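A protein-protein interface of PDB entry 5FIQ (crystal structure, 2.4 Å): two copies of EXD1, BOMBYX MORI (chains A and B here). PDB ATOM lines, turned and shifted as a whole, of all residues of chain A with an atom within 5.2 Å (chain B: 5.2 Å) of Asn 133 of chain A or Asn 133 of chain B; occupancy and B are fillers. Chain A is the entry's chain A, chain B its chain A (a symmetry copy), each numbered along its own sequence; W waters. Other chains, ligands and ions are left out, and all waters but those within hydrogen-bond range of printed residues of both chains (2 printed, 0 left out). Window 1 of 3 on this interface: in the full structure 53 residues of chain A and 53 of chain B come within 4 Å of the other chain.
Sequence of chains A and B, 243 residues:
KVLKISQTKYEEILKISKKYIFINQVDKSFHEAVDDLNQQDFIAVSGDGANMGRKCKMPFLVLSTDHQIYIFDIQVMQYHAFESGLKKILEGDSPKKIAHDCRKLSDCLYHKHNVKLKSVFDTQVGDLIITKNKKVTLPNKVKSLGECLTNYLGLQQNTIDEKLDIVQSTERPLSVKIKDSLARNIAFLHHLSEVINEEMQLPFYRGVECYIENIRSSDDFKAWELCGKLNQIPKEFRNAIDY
OD1 of Asn 133 of chain A lies close to OD1 of Asn 133 of chain B (3.3 Å).
Asn 133 of chain B touches Lys 132 of chain A (O to NZ, 3.6 Å). Lys 132 of chain B touches Asn 133 of chain A. CG2 of Val 136 of chain A touches CG2 of Val 136 of chain B, at 3.5 Å.
Of the printed residues of chain B, Asn 133 of chain A touches Lys 132 and Asn 133. Of chain A, only Lys 132 (3.6 Å) and Asn 133 (3.3 Å) come within 4 Å of Asn 133 of chain B. Of the printed residues of chain B, Val 136 of chain A touches Val 136. Printed residues of chain A within 4 Å of Lys 132 of chain B: Asn 133 (3.6 Å). Of the printed residues of chain A, Val 136 of chain B touches Val 136 (3.5 Å). Printed residues of chain B within 4 Å of Lys 132 of chain A: Asn 133. Ile 129 of chain B touches none of the printed residues of chain A. The nearest printed residue of chain A that does not touch Asn 133 of chain B is Ile 129 of chain A (6.1 Å). The nearest printed residue of chain B that does not touch Lys 132 of chain A is Lys 134 of chain B (5.2 Å).
Hydrophobic or aromatic side chains of chain B that line the printed part of chain A: Val 136. Along chain A the printed residues that touch a printed residue of chain B span positions 132 to 136. Among the printed residues, 4 pairs touch across the chains. Among the printed residues, no Asp or Glu carboxylate lies within 4 Å of a Lys or Arg side-chain nitrogen of the other chain.
Lys 132 of chain A touches Asn 133 of chain B, and with the chains exchanged Asn 133 of chain A touches Lys 132 of chain B. Asn 133 of chain B touches its own counterpart, Asn 133 of chain A. Val 136 of chain A touches its own counterpart, Val 136 of chain B. Positions printed for both chains: 128, 129, 130, 131, 132, 133, 134, 135, 136 and 200. Of the 4 pairs that touch across the chains among the printed residues, 4 have their exchanged pair printed and touching as well.
Water W2 lies within hydrogen-bond range of ND2 of Asn 133 of chain A (3.2 Å) and ND2 of Asn 133 of chain B (3.4 Å). Water W1 bridges ND2 of Asn 133 of chain B (3.2 Å) and ND2 of Asn 133 of chain A (3.4 Å).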
ATOM      1  N   LEU A 128     -14.639  10.891  19.474  1.00  0.00           N
ATOM      2  CA  LEU A 128     -14.118   9.512  19.595  1.00  0.00           C
ATOM      3  C   LEU A 128     -12.783   9.359  20.326  1.00  0.00           C
ATOM      4  O   LEU A 128     -12.622   8.468  21.134  1.00  0.00           O
ATOM      5  CB  LEU A 128     -13.967   8.833  18.231  1.00  0.00           C
ATOM      6  CG  LEU A 128     -15.339   8.710  17.536  1.00  0.00           C
ATOM      7  CD1 LEU A 128     -15.006   8.261  16.140  1.00  0.00           C
ATOM      8  CD2 LEU A 128     -16.251   7.743  18.248  1.00  0.00           C
ATOM      9  N   ILE A 129     -11.856  10.247  20.075  1.00  0.00           N
ATOM     10  CA  ILE A 129     -10.555  10.122  20.679  1.00  0.00           C
ATOM     11  C   ILE A 129     -10.655  10.457  22.152  1.00  0.00           C
ATOM     12  O   ILE A 129     -10.229   9.697  23.018  1.00  0.00           O
ATOM     13  CB  ILE A 129      -9.551  11.059  20.002  1.00  0.00           C
ATOM     14  CG1 ILE A 129      -9.376  10.707  18.540  1.00  0.00           C
ATOM     15  CG2 ILE A 129      -8.172  11.042  20.744  1.00  0.00           C
ATOM     16  CD1 ILE A 129      -8.671   9.419  18.268  1.00  0.00           C
ATOM     17  N   ILE A 130     -11.259  11.577  22.429  1.00  0.00           N
ATOM     18  CA  ILE A 130     -11.578  11.938  23.838  1.00  0.00           C
ATOM     19  C   ILE A 130     -12.288  10.817  24.562  1.00  0.00           C
ATOM     20  O   ILE A 130     -11.831  10.454  25.638  1.00  0.00           O
ATOM     21  CB  ILE A 130     -12.493  13.149  23.972  1.00  0.00           C
ATOM     22  CG1 ILE A 130     -11.772  14.374  23.481  1.00  0.00           C
ATOM     23  CG2 ILE A 130     -12.850  13.373  25.421  1.00  0.00           C
ATOM     24  CD1 ILE A 130     -12.703  15.493  23.111  1.00  0.00           C
ATOM     25  N   THR A 131     -13.315  10.210  23.974  1.00  0.00           N
ATOM     26  CA  THR A 131     -14.014   9.105  24.662  1.00  0.00           C
ATOM     27  C   THR A 131     -13.036   7.912  24.811  1.00  0.00           C
ATOM     28  O   THR A 131     -12.884   7.395  25.894  1.00  0.00           O
ATOM     29  CB  THR A 131     -15.347   8.678  23.970  1.00  0.00           C
ATOM     30  OG1 THR A 131     -16.295   9.789  23.890  1.00  0.00           O
ATOM     31  CG2 THR A 131     -15.978   7.537  24.727  1.00  0.00           C
ATOM     32  N   LYS A 132     -12.356   7.510  23.747  1.00  0.00           N
ATOM     33  CA  LYS A 132     -11.405   6.392  23.822  1.00  0.00           C
ATOM     34  C   LYS A 132     -10.349   6.597  24.864  1.00  0.00           C
ATOM     35  O   LYS A 132     -10.068   5.684  25.600  1.00  0.00           O
ATOM     36  CB  LYS A 132     -10.693   6.136  22.512  1.00  0.00           C
ATOM     37  CG  LYS A 132      -9.633   5.035  22.602  1.00  0.00           C
ATOM     38  CD  LYS A 132      -9.234   4.443  21.248  1.00  0.00           C
ATOM     39  CE  LYS A 132      -8.434   3.138  21.357  1.00  0.00           C
ATOM     40  NZ  LYS A 132      -7.086   3.452  21.870  1.00  0.00           N
ATOM     41  N   ASN A 133      -9.763   7.787  24.943  1.00  0.00           N
ATOM     42  CA  ASN A 133      -8.716   8.065  25.982  1.00  0.00           C
ATOM     43  C   ASN A 133      -9.278   8.149  27.379  1.00  0.00           C
ATOM     44  O   ASN A 133      -8.585   7.859  28.309  1.00  0.00           O
ATOM     45  CB  ASN A 133      -7.926   9.366  25.704  1.00  0.00           C
ATOM     46  CG  ASN A 133      -7.063   9.283  24.422  1.00  0.00           C
ATOM     47  OD1 ASN A 133      -6.860   8.225  23.846  1.00  0.00           O
ATOM     48  ND2 ASN A 133      -6.608  10.436  23.968  1.00  0.00           N
ATOM     49  N   LYS A 134     -10.532   8.546  27.529  1.00  0.00           N
ATOM     50  CA  LYS A 134     -11.095   8.609  28.854  1.00  0.00           C
ATOM     51  C   LYS A 134     -11.481   7.200  29.288  1.00  0.00           C
ATOM     52  O   LYS A 134     -10.852   6.657  30.150  1.00  0.00           O
ATOM     53  CB  LYS A 134     -12.298   9.556  28.919  1.00  0.00           C
ATOM     54  CG  LYS A 134     -12.549  10.068  30.315  1.00  0.00           C
ATOM     55  CD  LYS A 134     -13.581  11.178  30.270  1.00  0.00           C
ATOM     56  CE  LYS A 134     -12.930  12.535  29.999  1.00  0.00           C
ATOM     57  NZ  LYS A 134     -13.749  13.372  29.075  1.00  0.00           N
ATOM     58  N   LYS A 135     -12.497   6.615  28.644  1.00  0.00           N
ATOM     59  CA  LYS A 135     -13.143   5.364  29.081  1.00  0.00           C
ATOM     60  C   LYS A 135     -12.499   4.134  28.496  1.00  0.00           C
ATOM     61  O   LYS A 135     -13.165   3.112  28.358  1.00  0.00           O
ATOM     62  CB  LYS A 135     -14.605   5.370  28.670  1.00  0.00           C
ATOM     63  CG  LYS A 135     -15.338   6.593  29.149  1.00  0.00           C
ATOM     64  CD  LYS A 135     -16.821   6.483  28.860  1.00  0.00           C
ATOM     65  CE  LYS A 135     -17.579   7.578  29.595  1.00  0.00           C
ATOM     66  NZ  LYS A 135     -19.043   7.525  29.308  1.00  0.00           N
ATOM     67  N   VAL A 136     -11.240   4.269  28.066  1.00  0.00           N
ATOM     68  CA  VAL A 136     -10.328   3.172  27.633  1.00  0.00           C
ATOM     69  C   VAL A 136     -10.740   2.415  26.347  1.00  0.00           C
ATOM     70  O   VAL A 136      -9.944   2.253  25.405  1.00  0.00           O
ATOM     71  CB  VAL A 136      -9.987   2.231  28.826  1.00  0.00           C
ATOM     72  CG1 VAL A 136     -10.592   0.826  28.707  1.00  0.00           C
ATOM     73  CG2 VAL A 136      -8.469   2.137  28.985  1.00  0.00           C
ATOM     74  N   MET A 200      -8.920  16.915  23.979  1.00  0.00           N
ATOM     75  CA  MET A 200      -7.976  15.914  23.479  1.00  0.00           C
ATOM     76  C   MET A 200      -6.590  16.075  24.081  1.00  0.00           C
ATOM     77  O   MET A 200      -5.988  15.099  24.316  1.00  0.00           O
ATOM     78  CB  MET A 200      -7.748  15.959  21.984  1.00  0.00           C
ATOM     79  CG  MET A 200      -8.860  15.302  21.269  1.00  0.00           C
ATOM     80  SD  MET A 200      -8.468  15.080  19.541  1.00  0.00           S
ATOM     81  CE  MET A 200      -8.540  16.791  19.030  1.00  0.00           C
ATOM     82  N   LEU B 128       4.845   8.759  28.213  1.00  0.00           N
ATOM     83  CA  LEU B 128       3.713   8.190  28.978  1.00  0.00           C
ATOM     84  C   LEU B 128       2.346   8.241  28.294  1.00  0.00           C
ATOM     85  O   LEU B 128       1.605   7.280  28.328  1.00  0.00           O
ATOM     86  CB  LEU B 128       3.557   8.851  30.350  1.00  0.00           C
ATOM     87  CG  LEU B 128       4.814   8.611  31.210  1.00  0.00           C
ATOM     88  CD1 LEU B 128       4.621   9.505  32.404  1.00  0.00           C
ATOM     89  CD2 LEU B 128       4.969   7.162  31.597  1.00  0.00           C
ATOM     90  N   ILE B 129       2.039   9.334  27.644  1.00  0.00           N
ATOM     91  CA  ILE B 129       0.743   9.472  27.034  1.00  0.00           C
ATOM     92  C   ILE B 129       0.667   8.575  25.816  1.00  0.00           C
ATOM     93  O   ILE B 129      -0.249   7.772  25.661  1.00  0.00           O
ATOM     94  CB  ILE B 129       0.487  10.925  26.625  1.00  0.00           C
ATOM     95  CG1 ILE B 129       0.488  11.839  27.831  1.00  0.00           C
ATOM     96  CG2 ILE B 129      -0.854  11.061  25.829  1.00  0.00           C
ATOM     97  CD1 ILE B 129      -0.670  11.681  28.760  1.00  0.00           C
ATOM     98  N   ILE B 130       1.657   8.689  24.979  1.00  0.00           N
ATOM     99  CA  ILE B 130       1.794   7.746  23.834  1.00  0.00           C
ATOM    100  C   ILE B 130       1.700   6.303  24.276  1.00  0.00           C
ATOM    101  O   ILE B 130       0.903   5.580  23.693  1.00  0.00           O
ATOM    102  CB  ILE B 130       3.124   7.858  23.099  1.00  0.00           C
ATOM    103  CG1 ILE B 130       3.207   9.200  22.423  1.00  0.00           C
ATOM    104  CG2 ILE B 130       3.218   6.797  22.031  1.00  0.00           C
ATOM    105  CD1 ILE B 130       4.616   9.606  22.099  1.00  0.00           C
ATOM    106  N   THR B 131       2.410   5.897  25.325  1.00  0.00           N
ATOM    107  CA  THR B 131       2.323   4.492  25.777  1.00  0.00           C
ATOM    108  C   THR B 131       0.887   4.223  26.293  1.00  0.00           C
ATOM    109  O   THR B 131       0.273   3.266  25.880  1.00  0.00           O
ATOM    110  CB  THR B 131       3.401   4.107  26.839  1.00  0.00           C
ATOM    111  OG1 THR B 131       4.758   4.299  26.326  1.00  0.00           O
ATOM    112  CG2 THR B 131       3.224   2.669  27.253  1.00  0.00           C
ATOM    113  N   LYS B 132       0.348   5.077  27.151  1.00  0.00           N
ATOM    114  CA  LYS B 132      -1.013   4.886  27.672  1.00  0.00           C
ATOM    115  C   LYS B 132      -2.039   4.776  26.587  1.00  0.00           C
ATOM    116  O   LYS B 132      -2.878   3.911  26.658  1.00  0.00           O
ATOM    117  CB  LYS B 132      -1.454   6.004  28.590  1.00  0.00           C
ATOM    118  CG  LYS B 132      -2.903   5.864  29.063  1.00  0.00           C
ATOM    119  CD  LYS B 132      -3.231   6.684  30.314  1.00  0.00           C
ATOM    120  CE  LYS B 132      -4.561   6.297  30.974  1.00  0.00           C
ATOM    121  NZ  LYS B 132      -5.668   6.754  30.111  1.00  0.00           N
ATOM    122  N   ASN B 133      -1.983   5.636  25.576  1.00  0.00           N
ATOM    123  CA  ASN B 133      -2.965   5.564  24.443  1.00  0.00           C
ATOM    124  C   ASN B 133      -2.752   4.365  23.553  1.00  0.00           C
ATOM    125  O   ASN B 133      -3.684   3.895  22.969  1.00  0.00           O
ATOM    126  CB  ASN B 133      -2.951   6.830  23.554  1.00  0.00           C
ATOM    127  CG  ASN B 133      -3.444   8.093  24.299  1.00  0.00           C
ATOM    128  OD1 ASN B 133      -3.999   8.029  25.386  1.00  0.00           O
ATOM    129  ND2 ASN B 133      -3.178   9.242  23.707  1.00  0.00           N
ATOM    130  N   LYS B 134      -1.529   3.870  23.447  1.00  0.00           N
ATOM    131  CA  LYS B 134      -1.310   2.709  22.621  1.00  0.00           C
ATOM    132  C   LYS B 134      -1.754   1.471  23.391  1.00  0.00           C
ATOM    133  O   LYS B 134      -2.737   0.883  23.043  1.00  0.00           O
ATOM    134  CB  LYS B 134       0.152   2.590  22.180  1.00  0.00           C
ATOM    135  CG  LYS B 134       0.307   1.770  20.924  1.00  0.00           C
ATOM    136  CD  LYS B 134       1.727   1.897  20.406  1.00  0.00           C
ATOM    137  CE  LYS B 134       1.884   3.122  19.504  1.00  0.00           C
ATOM    138  NZ  LYS B 134       3.184   3.818  19.731  1.00  0.00           N
ATOM    139  N   LYS B 135      -1.031   1.120  24.460  1.00  0.00           N
ATOM    140  CA  LYS B 135      -1.179  -0.161  25.174  1.00  0.00           C
ATOM    141  C   LYS B 135      -2.189  -0.100  26.290  1.00  0.00           C
ATOM    142  O   LYS B 135      -2.083  -0.867  27.242  1.00  0.00           O
ATOM    143  CB  LYS B 135       0.156  -0.574  25.771  1.00  0.00           C
ATOM    144  CG  LYS B 135       1.261  -0.608  24.751  1.00  0.00           C
ATOM    145  CD  LYS B 135       2.531  -1.177  25.349  1.00  0.00           C
ATOM    146  CE  LYS B 135       3.540  -1.470  24.249  1.00  0.00           C
ATOM    147  NZ  LYS B 135       4.822  -2.002  24.802  1.00  0.00           N
ATOM    148  N   VAL B 136      -3.100   0.877  26.215  1.00  0.00           N
ATOM    149  CA  VAL B 136      -4.307   1.032  27.077  1.00  0.00           C
ATOM    150  C   VAL B 136      -4.039   1.327  28.572  1.00  0.00           C
ATOM    151  O   VAL B 136      -4.587   2.280  29.155  1.00  0.00           O
ATOM    152  CB  VAL B 136      -5.308  -0.137  26.842  1.00  0.00           C
ATOM    153  CG1 VAL B 136      -5.443  -1.093  28.035  1.00  0.00           C
ATOM    154  CG2 VAL B 136      -6.678   0.432  26.468  1.00  0.00           C
ATOM    155  N   MET B 200       1.896  11.576  19.690  1.00  0.00           N
ATOM    156  CA  MET B 200       0.722  11.844  20.522  1.00  0.00           C
ATOM    157  C   MET B 200      -0.509  12.177  19.696  1.00  0.00           C
ATOM    158  O   MET B 200      -1.541  11.782  20.084  1.00  0.00           O
ATOM    159  CB  MET B 200       0.877  13.020  21.463  1.00  0.00           C
ATOM    160  CG  MET B 200       1.662  12.633  22.652  1.00  0.00           C
ATOM    161  SD  MET B 200       1.599  13.908  23.902  1.00  0.00           S
ATOM    162  CE  MET B 200       2.594  15.141  23.074  1.00  0.00           C
HETATM  163  O   HOH W   1      -4.903   9.956  21.055  1.00  0.00           O
HETATM  164  O   HOH W   2      -4.220  11.836  25.660  1.00  0.00           O
